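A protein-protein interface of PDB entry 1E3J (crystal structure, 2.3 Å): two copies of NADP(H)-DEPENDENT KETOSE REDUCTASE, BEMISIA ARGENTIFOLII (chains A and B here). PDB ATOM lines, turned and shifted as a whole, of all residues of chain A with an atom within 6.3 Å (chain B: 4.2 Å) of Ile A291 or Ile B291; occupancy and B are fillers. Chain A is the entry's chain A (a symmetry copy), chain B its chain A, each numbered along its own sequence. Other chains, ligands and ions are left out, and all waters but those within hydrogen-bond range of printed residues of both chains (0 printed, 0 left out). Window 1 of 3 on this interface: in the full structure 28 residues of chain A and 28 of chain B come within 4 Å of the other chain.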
ATOM      1  N   ILE A 258      20.145  27.888  -8.468  1.00  0.00           N
ATOM      2  CA  ILE A 258      18.767  28.258  -8.709  1.00  0.00           C
ATOM      3  C   ILE A 258      18.303  29.412  -7.809  1.00  0.00           C
ATOM      4  O   ILE A 258      17.537  30.304  -8.232  1.00  0.00           O
ATOM      5  CB  ILE A 258      17.857  27.066  -8.415  1.00  0.00           C
ATOM      6  CG1 ILE A 258      18.142  25.954  -9.423  1.00  0.00           C
ATOM      7  CG2 ILE A 258      16.370  27.500  -8.440  1.00  0.00           C
ATOM      8  CD1 ILE A 258      17.376  24.685  -9.163  1.00  0.00           C
ATOM      9  N   GLY A 265      17.402  35.014 -15.559  1.00  0.00           N
ATOM     10  CA  GLY A 265      18.763  34.626 -15.876  1.00  0.00           C
ATOM     11  C   GLY A 265      18.817  33.154 -16.196  1.00  0.00           C
ATOM     12  O   GLY A 265      17.762  32.521 -16.374  1.00  0.00           O
ATOM     13  N   THR A 266      20.028  32.609 -16.226  1.00  0.00           N
ATOM     14  CA  THR A 266      20.220  31.233 -16.597  1.00  0.00           C
ATOM     15  C   THR A 266      21.216  30.460 -15.743  1.00  0.00           C
ATOM     16  O   THR A 266      22.213  31.006 -15.259  1.00  0.00           O
ATOM     17  CB  THR A 266      20.718  31.176 -18.067  1.00  0.00           C
ATOM     18  OG1 THR A 266      19.908  32.034 -18.868  1.00  0.00           O
ATOM     19  CG2 THR A 266      20.656  29.765 -18.612  1.00  0.00           C
ATOM     20  N   LEU A 267      20.928  29.176 -15.565  1.00  0.00           N
ATOM     21  CA  LEU A 267      21.816  28.294 -14.837  1.00  0.00           C
ATOM     22  C   LEU A 267      22.298  27.297 -15.872  1.00  0.00           C
ATOM     23  O   LEU A 267      21.475  26.580 -16.439  1.00  0.00           O
ATOM     24  CB  LEU A 267      21.014  27.575 -13.753  1.00  0.00           C
ATOM     25  CG  LEU A 267      21.746  26.406 -13.067  1.00  0.00           C
ATOM     26  CD1 LEU A 267      23.080  26.864 -12.510  1.00  0.00           C
ATOM     27  CD2 LEU A 267      20.855  25.865 -11.925  1.00  0.00           C
ATOM     28  N   MET A 268      23.601  27.276 -16.133  1.00  0.00           N
ATOM     29  CA  MET A 268      24.193  26.384 -17.096  1.00  0.00           C
ATOM     30  C   MET A 268      24.713  25.178 -16.320  1.00  0.00           C
ATOM     31  O   MET A 268      25.452  25.352 -15.342  1.00  0.00           O
ATOM     32  CB  MET A 268      25.385  27.027 -17.791  1.00  0.00           C
ATOM     33  CG  MET A 268      25.085  28.311 -18.507  1.00  0.00           C
ATOM     34  SD  MET A 268      23.769  28.043 -19.702  1.00  0.00           S
ATOM     35  CE  MET A 268      24.401  26.587 -20.618  1.00  0.00           C
ATOM     36  N   LEU A 269      24.318  23.974 -16.744  1.00  0.00           N
ATOM     37  CA  LEU A 269      24.767  22.729 -16.108  1.00  0.00           C
ATOM     38  C   LEU A 269      25.930  22.193 -16.928  1.00  0.00           C
ATOM     39  O   LEU A 269      25.760  21.825 -18.107  1.00  0.00           O
ATOM     40  CB  LEU A 269      23.661  21.682 -16.113  1.00  0.00           C
ATOM     41  CG  LEU A 269      22.424  22.159 -15.363  1.00  0.00           C
ATOM     42  CD1 LEU A 269      21.323  21.168 -15.583  1.00  0.00           C
ATOM     43  CD2 LEU A 269      22.751  22.326 -13.879  1.00  0.00           C
ATOM     44  N   LEU A 281      13.120  23.187  -8.361  1.00  0.00           N
ATOM     45  CA  LEU A 281      12.672  23.678  -9.656  1.00  0.00           C
ATOM     46  C   LEU A 281      11.532  24.676  -9.523  1.00  0.00           C
ATOM     47  O   LEU A 281      11.443  25.613 -10.323  1.00  0.00           O
ATOM     48  CB  LEU A 281      12.218  22.537 -10.569  1.00  0.00           C
ATOM     49  CG  LEU A 281      13.242  21.526 -11.073  1.00  0.00           C
ATOM     50  CD1 LEU A 281      12.602  20.775 -12.255  1.00  0.00           C
ATOM     51  CD2 LEU A 281      14.539  22.215 -11.495  1.00  0.00           C
ATOM     52  N   ALA A 284      12.674  28.122  -9.532  1.00  0.00           N
ATOM     53  CA  ALA A 284      13.176  28.553 -10.831  1.00  0.00           C
ATOM     54  C   ALA A 284      12.027  29.090 -11.667  1.00  0.00           C
ATOM     55  O   ALA A 284      12.122  30.155 -12.279  1.00  0.00           O
ATOM     56  CB  ALA A 284      13.848  27.377 -11.565  1.00  0.00           C
ATOM     57  N   ILE A 289      13.799  31.291 -14.335  1.00  0.00           N
ATOM     58  CA  ILE A 289      15.226  30.997 -14.461  1.00  0.00           C
ATOM     59  C   ILE A 289      15.221  29.830 -15.460  1.00  0.00           C
ATOM     60  O   ILE A 289      14.440  28.887 -15.299  1.00  0.00           O
ATOM     61  CB  ILE A 289      15.830  30.396 -13.169  1.00  0.00           C
ATOM     62  CG1 ILE A 289      15.653  31.349 -11.974  1.00  0.00           C
ATOM     63  CG2 ILE A 289      17.304  30.026 -13.399  1.00  0.00           C
ATOM     64  CD1 ILE A 289      16.479  32.594 -12.018  1.00  0.00           C
ATOM     65  N   ASP A 290      16.048  29.889 -16.486  1.00  0.00           N
ATOM     66  CA  ASP A 290      16.140  28.793 -17.402  1.00  0.00           C
ATOM     67  C   ASP A 290      17.317  27.921 -16.952  1.00  0.00           C
ATOM     68  O   ASP A 290      18.305  28.426 -16.419  1.00  0.00           O
ATOM     69  CB  ASP A 290      16.403  29.283 -18.822  1.00  0.00           C
ATOM     70  CG  ASP A 290      15.199  30.042 -19.429  1.00  0.00           C
ATOM     71  OD1 ASP A 290      14.042  29.891 -18.954  1.00  0.00           O
ATOM     72  OD2 ASP A 290      15.418  30.797 -20.401  1.00  0.00           O
ATOM     73  N   ILE A 291      17.197  26.610 -17.135  1.00  0.00           N
ATOM     74  CA  ILE A 291      18.269  25.703 -16.792  1.00  0.00           C
ATOM     75  C   ILE A 291      18.725  25.058 -18.107  1.00  0.00           C
ATOM     76  O   ILE A 291      17.971  24.296 -18.727  1.00  0.00           O
ATOM     77  CB  ILE A 291      17.795  24.632 -15.818  1.00  0.00           C
ATOM     78  CG1 ILE A 291      17.296  25.300 -14.523  1.00  0.00           C
ATOM     79  CG2 ILE A 291      18.935  23.643 -15.550  1.00  0.00           C
ATOM     80  CD1 ILE A 291      16.324  24.454 -13.723  1.00  0.00           C
ATOM     81  N   LYS A 292      19.944  25.374 -18.537  1.00  0.00           N
ATOM     82  CA  LYS A 292      20.461  24.848 -19.810  1.00  0.00           C
ATOM     83  C   LYS A 292      21.667  23.968 -19.633  1.00  0.00           C
ATOM     84  O   LYS A 292      22.559  24.257 -18.836  1.00  0.00           O
ATOM     85  CB  LYS A 292      20.830  25.989 -20.767  1.00  0.00           C
ATOM     86  CG  LYS A 292      19.678  26.901 -21.105  1.00  0.00           C
ATOM     87  CD  LYS A 292      20.074  27.880 -22.200  1.00  0.00           C
ATOM     88  CE  LYS A 292      18.912  28.798 -22.549  1.00  0.00           C
ATOM     89  NZ  LYS A 292      19.289  29.799 -23.581  1.00  0.00           N
ATOM     90  N   SER A 293      21.688  22.885 -20.393  1.00  0.00           N
ATOM     91  CA  SER A 293      22.777  21.932 -20.349  1.00  0.00           C
ATOM     92  C   SER A 293      23.792  22.318 -21.398  1.00  0.00           C
ATOM     93  O   SER A 293      23.475  22.946 -22.410  1.00  0.00           O
ATOM     94  CB  SER A 293      22.267  20.545 -20.688  1.00  0.00           C
ATOM     95  OG  SER A 293      20.993  20.326 -20.131  1.00  0.00           O
ATOM     96  N   LEU B 267      12.027  21.316 -22.174  1.00  0.00           N
ATOM     97  CA  LEU B 267      10.999  20.945 -21.224  1.00  0.00           C
ATOM     98  C   LEU B 267      10.552  22.259 -20.612  1.00  0.00           C
ATOM     99  O   LEU B 267      11.372  22.941 -19.997  1.00  0.00           O
ATOM    100  CB  LEU B 267      11.622  20.054 -20.149  1.00  0.00           C
ATOM    101  CG  LEU B 267      10.730  19.794 -18.920  1.00  0.00           C
ATOM    102  CD1 LEU B 267       9.384  19.237 -19.344  1.00  0.00           C
ATOM    103  CD2 LEU B 267      11.448  18.788 -17.990  1.00  0.00           C
ATOM    104  N   LEU B 269       8.379  24.207 -17.899  1.00  0.00           N
ATOM    105  CA  LEU B 269       7.767  23.994 -16.580  1.00  0.00           C
ATOM    106  C   LEU B 269       6.660  25.024 -16.422  1.00  0.00           C
ATOM    107  O   LEU B 269       6.924  26.241 -16.380  1.00  0.00           O
ATOM    108  CB  LEU B 269       8.781  24.212 -15.465  1.00  0.00           C
ATOM    109  CG  LEU B 269       9.964  23.260 -15.579  1.00  0.00           C
ATOM    110  CD1 LEU B 269      11.001  23.668 -14.578  1.00  0.00           C
ATOM    111  CD2 LEU B 269       9.496  21.822 -15.360  1.00  0.00           C
ATOM    112  N   LEU B 281      18.521  15.542 -13.617  1.00  0.00           N
ATOM    113  CA  LEU B 281      19.143  16.601 -14.399  1.00  0.00           C
ATOM    114  C   LEU B 281      20.337  16.096 -15.193  1.00  0.00           C
ATOM    115  O   LEU B 281      20.585  16.584 -16.300  1.00  0.00           O
ATOM    116  CB  LEU B 281      19.600  17.764 -13.517  1.00  0.00           C
ATOM    117  CG  LEU B 281      18.557  18.618 -12.801  1.00  0.00           C
ATOM    118  CD1 LEU B 281      19.258  19.911 -12.346  1.00  0.00           C
ATOM    119  CD2 LEU B 281      17.372  18.926 -13.715  1.00  0.00           C
ATOM    120  N   ILE B 289      19.130  18.967 -23.090  1.00  0.00           N
ATOM    121  CA  ILE B 289      17.705  19.285 -22.996  1.00  0.00           C
ATOM    122  C   ILE B 289      17.724  20.573 -22.160  1.00  0.00           C
ATOM    123  O   ILE B 289      18.406  20.630 -21.132  1.00  0.00           O
ATOM    124  CB  ILE B 289      16.921  18.273 -22.127  1.00  0.00           C
ATOM    125  CG1 ILE B 289      17.045  16.844 -22.684  1.00  0.00           C
ATOM    126  CG2 ILE B 289      15.455  18.716 -21.995  1.00  0.00           C
ATOM    127  CD1 ILE B 289      16.331  16.594 -23.973  1.00  0.00           C
ATOM    128  N   ASP B 290      17.018  21.602 -22.591  1.00  0.00           N
ATOM    129  CA  ASP B 290      16.937  22.798 -21.809  1.00  0.00           C
ATOM    130  C   ASP B 290      15.654  22.714 -20.977  1.00  0.00           C
ATOM    131  O   ASP B 290      14.658  22.138 -21.416  1.00  0.00           O
ATOM    132  CB  ASP B 290      16.867  24.034 -22.701  1.00  0.00           C
ATOM    133  CG  ASP B 290      18.186  24.300 -23.466  1.00  0.00           C
ATOM    134  OD1 ASP B 290      19.270  23.797 -23.067  1.00  0.00           O
ATOM    135  OD2 ASP B 290      18.132  25.028 -24.481  1.00  0.00           O
ATOM    136  N   ILE B 291      15.688  23.256 -19.764  1.00  0.00           N
ATOM    137  CA  ILE B 291      14.516  23.275 -18.917  1.00  0.00           C
ATOM    138  C   ILE B 291      14.154  24.751 -18.717  1.00  0.00           C
ATOM    139  O   ILE B 291      14.906  25.502 -18.082  1.00  0.00           O
ATOM    140  CB  ILE B 291      14.797  22.616 -17.573  1.00  0.00           C
ATOM    141  CG1 ILE B 291      15.207  21.147 -17.797  1.00  0.00           C
ATOM    142  CG2 ILE B 291      13.561  22.734 -16.676  1.00  0.00           C
ATOM    143  CD1 ILE B 291      16.018  20.550 -16.662  1.00  0.00           C
ATOM    144  N   LYS B 292      13.017  25.168 -19.268  1.00  0.00           N
ATOM    145  CA  LYS B 292      12.598  26.575 -19.176  1.00  0.00           C
ATOM    146  C   LYS B 292      11.314  26.755 -18.416  1.00  0.00           C
ATOM    147  O   LYS B 292      10.367  25.983 -18.564  1.00  0.00           O
ATOM    148  CB  LYS B 292      12.425  27.190 -20.571  1.00  0.00           C
ATOM    149  CG  LYS B 292      13.675  27.159 -21.413  1.00  0.00           C
ATOM    150  CD  LYS B 292      13.478  27.954 -22.694  1.00  0.00           C
ATOM    151  CE  LYS B 292      14.740  27.930 -23.545  1.00  0.00           C
ATOM    152  NZ  LYS B 292      14.556  28.657 -24.828  1.00  0.00           N
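The backbone carbonyl oxygen of Ile B289 lies within hydrogen-bond range of the side-chain hydroxyl of Ser A293 (2.8 Å). O of Ile A291 sits at hydrogen-bond distance from N of Ile B291.
The backbone NH (N) of Leu B267 is in hydrogen-bond range of the backbone carbonyl oxygen (O) of Asp B290 (2.9 Å). The backbone NH (N) of Lys B292 lies within hydrogen-bond range of the backbone carbonyl oxygen (O) of Leu B267 (2.9 Å). The backbone carbonyl oxygen of Lys B292 is in hydrogen-bond range of the backbone NH of Leu B269 (2.7 Å). The backbone carbonyl oxygen (O) of Gly A265 lies within hydrogen-bond range of the backbone NH (N) of Asp A290 (3.1 Å). O of Asp A290 is in hydrogen-bond range of N of Leu A267 (2.9 Å). N of Lys A292 sits at hydrogen-bond distance from O of Leu A267 (2.9 Å).
Ile B291 touches Asp A290. Asp A290 touches Lys B292. CA of Asp B290 touches O of Ile A291, at 3.6 Å. OD1 of Asp B290 touches CB of Lys A292, at 3.5 Å. Asp B290 touches Ser A293 (OD1 to N, 3.7 Å).
Ile B291 touches just these residues of chain A: Asp A290 and Ile A291. Printed residues of chain B within 4 Å of Lys A292: Asp B290. Printed residues of chain A within 4 Å of Lys B292: Asp A290. Printed residues of chain B within 4 Å of Ser A293: Ile B289 and Asp B290. Printed residues of chain A within 4 Å of Asp B290: Ile A291, Lys A292 and Ser A293. Printed residues of chain A within 4 Å of Ile B289: Ser A293 (2.8 Å). The nearest printed residue of chain B that does not touch Ile A291 is Ile B289 (4.4 Å). The nearest residue of chain A that does not touch Ile B291 is Ile A289 (4.4 Å).
Hydrophobic or aromatic side chains of chain B within 4 Å of the printed part of chain A: Ile B291. Among the printed residues, 7 pairs touch across the chains. Among the printed residues, no Asp or Glu carboxylate lies within 4 Å of a Lys or Arg side-chain nitrogen of the other chain.
Asp A290 touches Ile B291, and with the chains exchanged Ile A291 touches Asp B290. Asp A290 touches Lys B292, and with the chains exchanged Lys A292 touches Asp B290. Ile A291 touches its own counterpart, Ile B291. Of the 7 pairs that touch across the chains among the printed residues, 5 have their exchanged pair printed and touching as well.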
